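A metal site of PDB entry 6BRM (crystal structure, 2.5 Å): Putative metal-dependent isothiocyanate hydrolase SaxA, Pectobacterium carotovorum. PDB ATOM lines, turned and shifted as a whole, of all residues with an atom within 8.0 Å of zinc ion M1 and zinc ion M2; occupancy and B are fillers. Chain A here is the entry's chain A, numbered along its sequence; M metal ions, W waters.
Zinc ion M1 is bound by water W2 (2.2 Å), a ring nitrogen (ND1) of His 69 (2.2 Å), a ring nitrogen (NE2) of His 128 (2.2 Å), a ring nitrogen (NE2) of His 67 (2.2 Å) and the side-chain carboxylate (OD2) of Asp 164 (2.2 Å). Zinc ion M1 has five donor atoms within binding distance.
The side-chain carboxylate of Asp 164 is in hydrogen-bond range of the side-chain amide nitrogen of Asn 186. ND1 of His 72 lies within hydrogen-bond range of OD2 of Asp 23 (3.3 Å). NE2 of His 69 lies within hydrogen-bond range of O of Leu 142 (2.9 Å). A ring nitrogen (ND1) of His 128 lies within hydrogen-bond range of the backbone carbonyl oxygen (O) of Ile 198 (3.1 Å). O of Asp 71 sits close to OD1 of Asn 8. ND1 of His 67 sits at hydrogen-bond distance from OG1 of Thr 66 (3.0 Å). N of His 221 is in hydrogen-bond range of O of Asn 8, at 2.8 Å. The side-chain sulfur of Cys 228 sits at hydrogen-bond distance from a ring nitrogen (ND1) of His 221 (3.6 Å).
Of the 28 residues printed, 5 come within 4 Å of zinc ion M1. Along chain A the residues within 4 Å of zinc ion M1 span positions 67 to 164.
Four residues have an atom within 4 Å of zinc ion M2: Asp 71, His 72, Asp 164 and His 221. The nearest printed residue that does not touch zinc ion M2 is His 67 (4.3 Å).
Zinc ion M2 is bound by OD2 of Asp 164, at 2.2 Å. Zinc ion M2 is bound by a ring nitrogen (NE2) of His 72 (2.2 Å). Water W2 is bound to zinc ion M2 (2.2 Å). Zinc ion M2 is bound by water W1, 2.2 Å away. OD2 of Asp 71 binds zinc ion M2, at 2.2 Å. Zinc ion M2 is bound by NE2 of His 221 (2.2 Å). Zinc ion M2 has six donor atoms within binding distance.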
ATOM      1  N   ASN A   8      12.117 -15.256  13.063  1.00  0.00           N
ATOM      2  CA  ASN A   8      11.150 -14.512  13.877  1.00  0.00           C
ATOM      3  C   ASN A   8      10.029 -15.451  14.365  1.00  0.00           C
ATOM      4  O   ASN A   8      10.309 -16.315  15.187  1.00  0.00           O
ATOM      5  CB  ASN A   8      10.668 -13.242  13.164  1.00  0.00           C
ATOM      6  CG  ASN A   8       9.895 -12.309  14.090  1.00  0.00           C
ATOM      7  OD1 ASN A   8       8.730 -12.005  13.856  1.00  0.00           O
ATOM      8  ND2 ASN A   8      10.544 -11.851  15.148  1.00  0.00           N
ATOM      9  N   ALA A   9       8.795 -15.289  13.869  1.00  0.00           N
ATOM     10  CA  ALA A   9       7.671 -16.163  14.225  1.00  0.00           C
ATOM     11  C   ALA A   9       7.230 -17.047  13.046  1.00  0.00           C
ATOM     12  O   ALA A   9       6.208 -17.732  13.143  1.00  0.00           O
ATOM     13  CB  ALA A   9       6.500 -15.337  14.730  1.00  0.00           C
ATOM     14  N   ASP A  23       2.688 -17.586   9.713  1.00  0.00           N
ATOM     15  CA  ASP A  23       3.222 -16.215   9.690  1.00  0.00           C
ATOM     16  C   ASP A  23       4.480 -16.043   8.810  1.00  0.00           C
ATOM     17  O   ASP A  23       5.555 -15.730   9.316  1.00  0.00           O
ATOM     18  CB  ASP A  23       3.495 -15.745  11.130  1.00  0.00           C
ATOM     19  CG  ASP A  23       2.251 -15.786  12.014  1.00  0.00           C
ATOM     20  OD1 ASP A  23       1.141 -15.504  11.511  1.00  0.00           O
ATOM     21  OD2 ASP A  23       2.369 -16.103  13.216  1.00  0.00           O
ATOM     22  N   PHE A  35      10.836  -0.416  13.009  1.00  0.00           N
ATOM     23  CA  PHE A  35       9.551   0.077  13.523  1.00  0.00           C
ATOM     24  C   PHE A  35       9.691   1.432  14.229  1.00  0.00           C
ATOM     25  O   PHE A  35      10.455   1.562  15.180  1.00  0.00           O
ATOM     26  CB  PHE A  35       8.910  -0.939  14.483  1.00  0.00           C
ATOM     27  CG  PHE A  35       8.255  -2.100  13.794  1.00  0.00           C
ATOM     28  CD1 PHE A  35       6.975  -1.971  13.262  1.00  0.00           C
ATOM     29  CD2 PHE A  35       8.892  -3.336  13.686  1.00  0.00           C
ATOM     30  CE1 PHE A  35       6.348  -3.039  12.635  1.00  0.00           C
ATOM     31  CE2 PHE A  35       8.281  -4.407  13.063  1.00  0.00           C
ATOM     32  CZ  PHE A  35       7.006  -4.254  12.529  1.00  0.00           C
ATOM     33  N   THR A  66      -1.714 -15.444  11.850  1.00  0.00           N
ATOM     34  CA  THR A  66      -2.189 -15.028  13.179  1.00  0.00           C
ATOM     35  C   THR A  66      -2.633 -13.559  13.197  1.00  0.00           C
ATOM     36  O   THR A  66      -3.618 -13.214  13.845  1.00  0.00           O
ATOM     37  CB  THR A  66      -1.135 -15.257  14.276  1.00  0.00           C
ATOM     38  OG1 THR A  66       0.071 -14.545  13.947  1.00  0.00           O
ATOM     39  CG2 THR A  66      -0.820 -16.742  14.427  1.00  0.00           C
ATOM     40  N   HIS A  67      -1.883 -12.709  12.490  1.00  0.00           N
ATOM     41  CA  HIS A  67      -2.259 -11.307  12.246  1.00  0.00           C
ATOM     42  C   HIS A  67      -1.404 -10.716  11.116  1.00  0.00           C
ATOM     43  O   HIS A  67      -0.534 -11.411  10.589  1.00  0.00           O
ATOM     44  CB  HIS A  67      -2.198 -10.460  13.534  1.00  0.00           C
ATOM     45  CG  HIS A  67      -0.839 -10.424  14.183  1.00  0.00           C
ATOM     46  ND1 HIS A  67      -0.129 -11.560  14.503  1.00  0.00           N
ATOM     47  CD2 HIS A  67      -0.099  -9.376  14.604  1.00  0.00           C
ATOM     48  CE1 HIS A  67       1.010 -11.208  15.078  1.00  0.00           C
ATOM     49  NE2 HIS A  67       1.056  -9.887  15.148  1.00  0.00           N
ATOM     50  N   THR A  68      -1.671  -9.471  10.738  1.00  0.00           N
ATOM     51  CA  THR A  68      -1.058  -8.850   9.558  1.00  0.00           C
ATOM     52  C   THR A  68      -0.043  -7.731   9.880  1.00  0.00           C
ATOM     53  O   THR A  68       0.052  -6.749   9.137  1.00  0.00           O
ATOM     54  CB  THR A  68      -2.144  -8.288   8.624  1.00  0.00           C
ATOM     55  OG1 THR A  68      -2.842  -7.238   9.299  1.00  0.00           O
ATOM     56  CG2 THR A  68      -3.134  -9.380   8.225  1.00  0.00           C
ATOM     57  N   HIS A  69       0.707  -7.883  10.974  1.00  0.00           N
ATOM     58  CA  HIS A  69       1.908  -7.052  11.207  1.00  0.00           C
ATOM     59  C   HIS A  69       2.990  -7.500  10.221  1.00  0.00           C
ATOM     60  O   HIS A  69       2.998  -8.652   9.781  1.00  0.00           O
ATOM     61  CB  HIS A  69       2.418  -7.158  12.650  1.00  0.00           C
ATOM     62  CG  HIS A  69       1.583  -6.388  13.644  1.00  0.00           C
ATOM     63  ND1 HIS A  69       1.492  -6.748  14.971  1.00  0.00           N
ATOM     64  CD2 HIS A  69       0.830  -5.274  13.506  1.00  0.00           C
ATOM     65  CE1 HIS A  69       0.696  -5.897  15.601  1.00  0.00           C
ATOM     66  NE2 HIS A  69       0.286  -4.991  14.731  1.00  0.00           N
ATOM     67  N   THR A  70       3.897  -6.589   9.892  1.00  0.00           N
ATOM     68  CA  THR A  70       4.867  -6.803   8.820  1.00  0.00           C
ATOM     69  C   THR A  70       5.925  -7.893   9.097  1.00  0.00           C
ATOM     70  O   THR A  70       6.446  -8.499   8.162  1.00  0.00           O
ATOM     71  CB  THR A  70       5.583  -5.491   8.451  1.00  0.00           C
ATOM     72  OG1 THR A  70       4.616  -4.425   8.401  1.00  0.00           O
ATOM     73  CG2 THR A  70       6.272  -5.587   7.093  1.00  0.00           C
ATOM     74  N   ASP A  71       6.212  -8.164  10.369  1.00  0.00           N
ATOM     75  CA  ASP A  71       7.108  -9.288  10.758  1.00  0.00           C
ATOM     76  C   ASP A  71       6.434 -10.675  10.693  1.00  0.00           C
ATOM     77  O   ASP A  71       7.099 -11.690  10.903  1.00  0.00           O
ATOM     78  CB  ASP A  71       7.717  -9.067  12.146  1.00  0.00           C
ATOM     79  CG  ASP A  71       6.676  -8.866  13.225  1.00  0.00           C
ATOM     80  OD1 ASP A  71       5.824  -7.976  13.030  1.00  0.00           O
ATOM     81  OD2 ASP A  71       6.718  -9.561  14.246  1.00  0.00           O
ATOM     82  N   HIS A  72       5.118 -10.706  10.446  1.00  0.00           N
ATOM     83  CA  HIS A  72       4.359 -11.936  10.222  1.00  0.00           C
ATOM     84  C   HIS A  72       3.837 -12.096   8.774  1.00  0.00           C
ATOM     85  O   HIS A  72       3.432 -13.183   8.389  1.00  0.00           O
ATOM     86  CB  HIS A  72       3.176 -11.981  11.200  1.00  0.00           C
ATOM     87  CG  HIS A  72       3.600 -11.951  12.639  1.00  0.00           C
ATOM     88  ND1 HIS A  72       3.677 -13.078  13.421  1.00  0.00           N
ATOM     89  CD2 HIS A  72       3.972 -10.915  13.437  1.00  0.00           C
ATOM     90  CE1 HIS A  72       4.093 -12.744  14.630  1.00  0.00           C
ATOM     91  NE2 HIS A  72       4.278 -11.435  14.667  1.00  0.00           N
ATOM     92  N   HIS A 128      -1.991  -7.961  22.563  1.00  0.00           N
ATOM     93  CA  HIS A 128      -0.725  -7.610  21.928  1.00  0.00           C
ATOM     94  C   HIS A 128      -0.278  -6.232  22.438  1.00  0.00           C
ATOM     95  O   HIS A 128      -0.083  -5.295  21.671  1.00  0.00           O
ATOM     96  CB  HIS A 128      -0.928  -7.630  20.413  1.00  0.00           C
ATOM     97  CG  HIS A 128       0.344  -7.619  19.633  1.00  0.00           C
ATOM     98  ND1 HIS A 128       1.559  -7.239  20.171  1.00  0.00           N
ATOM     99  CD2 HIS A 128       0.580  -7.901  18.332  1.00  0.00           C
ATOM    100  CE1 HIS A 128       2.489  -7.312  19.236  1.00  0.00           C
ATOM    101  NE2 HIS A 128       1.929  -7.693  18.102  1.00  0.00           N
ATOM    102  N   LEU A 142      -3.684  -0.102  15.930  1.00  0.00           N
ATOM    103  CA  LEU A 142      -2.373  -0.424  15.353  1.00  0.00           C
ATOM    104  C   LEU A 142      -1.851  -1.794  15.845  1.00  0.00           C
ATOM    105  O   LEU A 142      -1.406  -2.615  15.039  1.00  0.00           O
ATOM    106  CB  LEU A 142      -1.355   0.685  15.633  1.00  0.00           C
ATOM    107  CG  LEU A 142      -0.309   0.951  14.536  1.00  0.00           C
ATOM    108  CD1 LEU A 142       0.349   2.303  14.754  1.00  0.00           C
ATOM    109  CD2 LEU A 142       0.725  -0.167  14.438  1.00  0.00           C
ATOM    110  N   LEU A 143      -1.914  -2.019  17.150  1.00  0.00           N
ATOM    111  CA  LEU A 143      -1.539  -3.318  17.733  1.00  0.00           C
ATOM    112  C   LEU A 143      -2.607  -4.387  17.445  1.00  0.00           C
ATOM    113  O   LEU A 143      -2.263  -5.529  17.101  1.00  0.00           O
ATOM    114  CB  LEU A 143      -1.262  -3.214  19.241  1.00  0.00           C
ATOM    115  CG  LEU A 143       0.138  -2.771  19.697  1.00  0.00           C
ATOM    116  CD1 LEU A 143       1.217  -3.739  19.222  1.00  0.00           C
ATOM    117  CD2 LEU A 143       0.454  -1.345  19.248  1.00  0.00           C
ATOM    118  N   GLY A 144      -3.872  -4.015  17.604  1.00  0.00           N
ATOM    119  CA  GLY A 144      -5.004  -4.815  17.136  1.00  0.00           C
ATOM    120  C   GLY A 144      -5.170  -6.166  17.807  1.00  0.00           C
ATOM    121  O   GLY A 144      -4.805  -6.330  18.976  1.00  0.00           O
ATOM    122  N   ASP A 145      -5.739  -7.118  17.065  1.00  0.00           N
ATOM    123  CA  ASP A 145      -5.860  -8.503  17.523  1.00  0.00           C
ATOM    124  C   ASP A 145      -4.711  -9.328  16.955  1.00  0.00           C
ATOM    125  O   ASP A 145      -4.165  -9.004  15.893  1.00  0.00           O
ATOM    126  CB  ASP A 145      -7.196  -9.102  17.069  1.00  0.00           C
ATOM    127  CG  ASP A 145      -8.398  -8.277  17.501  1.00  0.00           C
ATOM    128  OD1 ASP A 145      -8.247  -7.380  18.367  1.00  0.00           O
ATOM    129  OD2 ASP A 145      -9.494  -8.519  16.968  1.00  0.00           O
ATOM    130  N   ALA A 146      -4.360 -10.411  17.648  1.00  0.00           N
ATOM    131  CA  ALA A 146      -3.356 -11.358  17.177  1.00  0.00           C
ATOM    132  C   ALA A 146      -3.502 -12.707  17.889  1.00  0.00           C
ATOM    133  O   ALA A 146      -3.092 -12.844  19.043  1.00  0.00           O
ATOM    134  CB  ALA A 146      -1.953 -10.796  17.374  1.00  0.00           C
ATOM    135  N   GLY A 163       1.250 -16.969  20.018  1.00  0.00           N
ATOM    136  CA  GLY A 163       1.165 -15.729  19.215  1.00  0.00           C
ATOM    137  C   GLY A 163       1.651 -14.479  19.930  1.00  0.00           C
ATOM    138  O   GLY A 163       2.104 -14.543  21.072  1.00  0.00           O
ATOM    139  N   ASP A 164       1.560 -13.336  19.245  1.00  0.00           N
ATOM    140  CA  ASP A 164       1.937 -12.040  19.821  1.00  0.00           C
ATOM    141  C   ASP A 164       0.955 -11.609  20.904  1.00  0.00           C
ATOM    142  O   ASP A 164      -0.002 -10.879  20.651  1.00  0.00           O
ATOM    143  CB  ASP A 164       1.987 -10.950  18.736  1.00  0.00           C
ATOM    144  CG  ASP A 164       3.191 -11.066  17.808  1.00  0.00           C
ATOM    145  OD1 ASP A 164       3.853 -12.119  17.774  1.00  0.00           O
ATOM    146  OD2 ASP A 164       3.462 -10.071  17.103  1.00  0.00           O
ATOM    147  N   THR A 165       1.219 -12.070  22.132  1.00  0.00           N
ATOM    148  CA  THR A 165       0.421 -11.729  23.303  1.00  0.00           C
ATOM    149  C   THR A 165       1.312 -11.567  24.533  1.00  0.00           C
ATOM    150  O   THR A 165       2.337 -12.246  24.622  1.00  0.00           O
ATOM    151  CB  THR A 165      -0.657 -12.803  23.573  1.00  0.00           C
ATOM    152  OG1 THR A 165      -1.510 -12.376  24.642  1.00  0.00           O
ATOM    153  CG2 THR A 165      -0.043 -14.164  23.917  1.00  0.00           C
ATOM    154  N   ASN A 186       6.079 -16.423  21.790  1.00  0.00           N
ATOM    155  CA  ASN A 186       6.793 -15.335  21.138  1.00  0.00           C
ATOM    156  C   ASN A 186       7.469 -14.500  22.229  1.00  0.00           C
ATOM    157  O   ASN A 186       6.887 -13.556  22.759  1.00  0.00           O
ATOM    158  CB  ASN A 186       5.825 -14.497  20.281  1.00  0.00           C
ATOM    159  CG  ASN A 186       5.234 -15.299  19.140  1.00  0.00           C
ATOM    160  OD1 ASN A 186       5.441 -16.502  19.027  1.00  0.00           O
ATOM    161  ND2 ASN A 186       4.479 -14.629  18.283  1.00  0.00           N
ATOM    162  N   ALA A 190       9.585  -7.318  22.868  1.00  0.00           N
ATOM    163  CA  ALA A 190       9.532  -6.134  22.012  1.00  0.00           C
ATOM    164  C   ALA A 190       9.017  -4.943  22.801  1.00  0.00           C
ATOM    165  O   ALA A 190       7.935  -4.998  23.381  1.00  0.00           O
ATOM    166  CB  ALA A 190       8.667  -6.385  20.797  1.00  0.00           C
ATOM    167  N   ILE A 198       5.242  -5.233  24.420  1.00  0.00           N
ATOM    168  CA  ILE A 198       4.065  -5.602  23.613  1.00  0.00           C
ATOM    169  C   ILE A 198       3.872  -7.118  23.435  1.00  0.00           C
ATOM    170  O   ILE A 198       2.798  -7.551  23.044  1.00  0.00           O
ATOM    171  CB  ILE A 198       4.023  -4.902  22.227  1.00  0.00           C
ATOM    172  CG1 ILE A 198       5.179  -5.350  21.309  1.00  0.00           C
ATOM    173  CG2 ILE A 198       4.045  -3.394  22.404  1.00  0.00           C
ATOM    174  CD1 ILE A 198       5.072  -4.825  19.890  1.00  0.00           C
ATOM    175  N   ILE A 199       4.915  -7.900  23.713  1.00  0.00           N
ATOM    176  CA  ILE A 199       4.867  -9.375  23.717  1.00  0.00           C
ATOM    177  C   ILE A 199       5.689  -9.925  24.897  1.00  0.00           C
ATOM    178  O   ILE A 199       6.289  -9.155  25.650  1.00  0.00           O
ATOM    179  CB  ILE A 199       5.327  -9.978  22.367  1.00  0.00           C
ATOM    180  CG1 ILE A 199       6.785  -9.610  22.050  1.00  0.00           C
ATOM    181  CG2 ILE A 199       4.426  -9.509  21.222  1.00  0.00           C
ATOM    182  CD1 ILE A 199       7.363 -10.343  20.850  1.00  0.00           C
ATOM    183  N   HIS A 221      10.270 -15.798  17.987  1.00  0.00           N
ATOM    184  CA  HIS A 221      10.096 -14.342  17.804  1.00  0.00           C
ATOM    185  C   HIS A 221      11.301 -13.557  18.356  1.00  0.00           C
ATOM    186  O   HIS A 221      11.129 -12.483  18.934  1.00  0.00           O
ATOM    187  CB  HIS A 221       8.755 -13.861  18.416  1.00  0.00           C
ATOM    188  CG  HIS A 221       8.171 -12.650  17.745  1.00  0.00           C
ATOM    189  ND1 HIS A 221       8.827 -11.447  17.672  1.00  0.00           N
ATOM    190  CD2 HIS A 221       6.965 -12.461  17.157  1.00  0.00           C
ATOM    191  CE1 HIS A 221       8.059 -10.574  17.046  1.00  0.00           C
ATOM    192  NE2 HIS A 221       6.910 -11.157  16.733  1.00  0.00           N
ATOM    193  N   ILE A 225      13.670  -8.931  14.502  1.00  0.00           N
ATOM    194  CA  ILE A 225      13.073  -7.596  14.435  1.00  0.00           C
ATOM    195  C   ILE A 225      13.792  -6.673  15.403  1.00  0.00           C
ATOM    196  O   ILE A 225      14.260  -7.109  16.463  1.00  0.00           O
ATOM    197  CB  ILE A 225      11.555  -7.666  14.751  1.00  0.00           C
ATOM    198  CG1 ILE A 225      10.863  -8.717  13.861  1.00  0.00           C
ATOM    199  CG2 ILE A 225      10.888  -6.314  14.564  1.00  0.00           C
ATOM    200  CD1 ILE A 225      11.061  -8.536  12.364  1.00  0.00           C
ATOM    201  N   HIS A 227      13.023  -4.157  17.512  1.00  0.00           N
ATOM    202  CA  HIS A 227      12.573  -3.845  18.872  1.00  0.00           C
ATOM    203  C   HIS A 227      12.608  -5.027  19.854  1.00  0.00           C
ATOM    204  O   HIS A 227      12.447  -4.826  21.050  1.00  0.00           O
ATOM    205  CB  HIS A 227      11.204  -3.126  18.907  1.00  0.00           C
ATOM    206  CG  HIS A 227      10.092  -3.859  18.217  1.00  0.00           C
ATOM    207  ND1 HIS A 227      10.042  -5.231  18.122  1.00  0.00           N
ATOM    208  CD2 HIS A 227       8.959  -3.396  17.639  1.00  0.00           C
ATOM    209  CE1 HIS A 227       8.936  -5.581  17.489  1.00  0.00           C
ATOM    210  NE2 HIS A 227       8.266  -4.490  17.190  1.00  0.00           N
ATOM    211  N   CYS A 228      12.836  -6.244  19.347  1.00  0.00           N
ATOM    212  CA  CYS A 228      12.973  -7.429  20.206  1.00  0.00           C
ATOM    213  C   CYS A 228      14.352  -7.477  20.876  1.00  0.00           C
ATOM    214  O   CYS A 228      15.342  -7.831  20.246  1.00  0.00           O
ATOM    215  CB  CYS A 228      12.726  -8.700  19.394  1.00  0.00           C
ATOM    216  SG  CYS A 228      11.010  -8.868  18.854  1.00  0.00           S
HETATM  217 ZN    ZN M   1       2.415  -8.409  16.078  1.00  0.00          ZN
HETATM  218 ZN    ZN M   2       5.283  -9.912  15.891  1.00  0.00          ZN
HETATM  219  O   HOH W   1       6.117  -8.245  17.077  1.00  0.00           O
HETATM  220  O   HOH W   2       4.332  -8.100  15.076  1.00  0.00           O
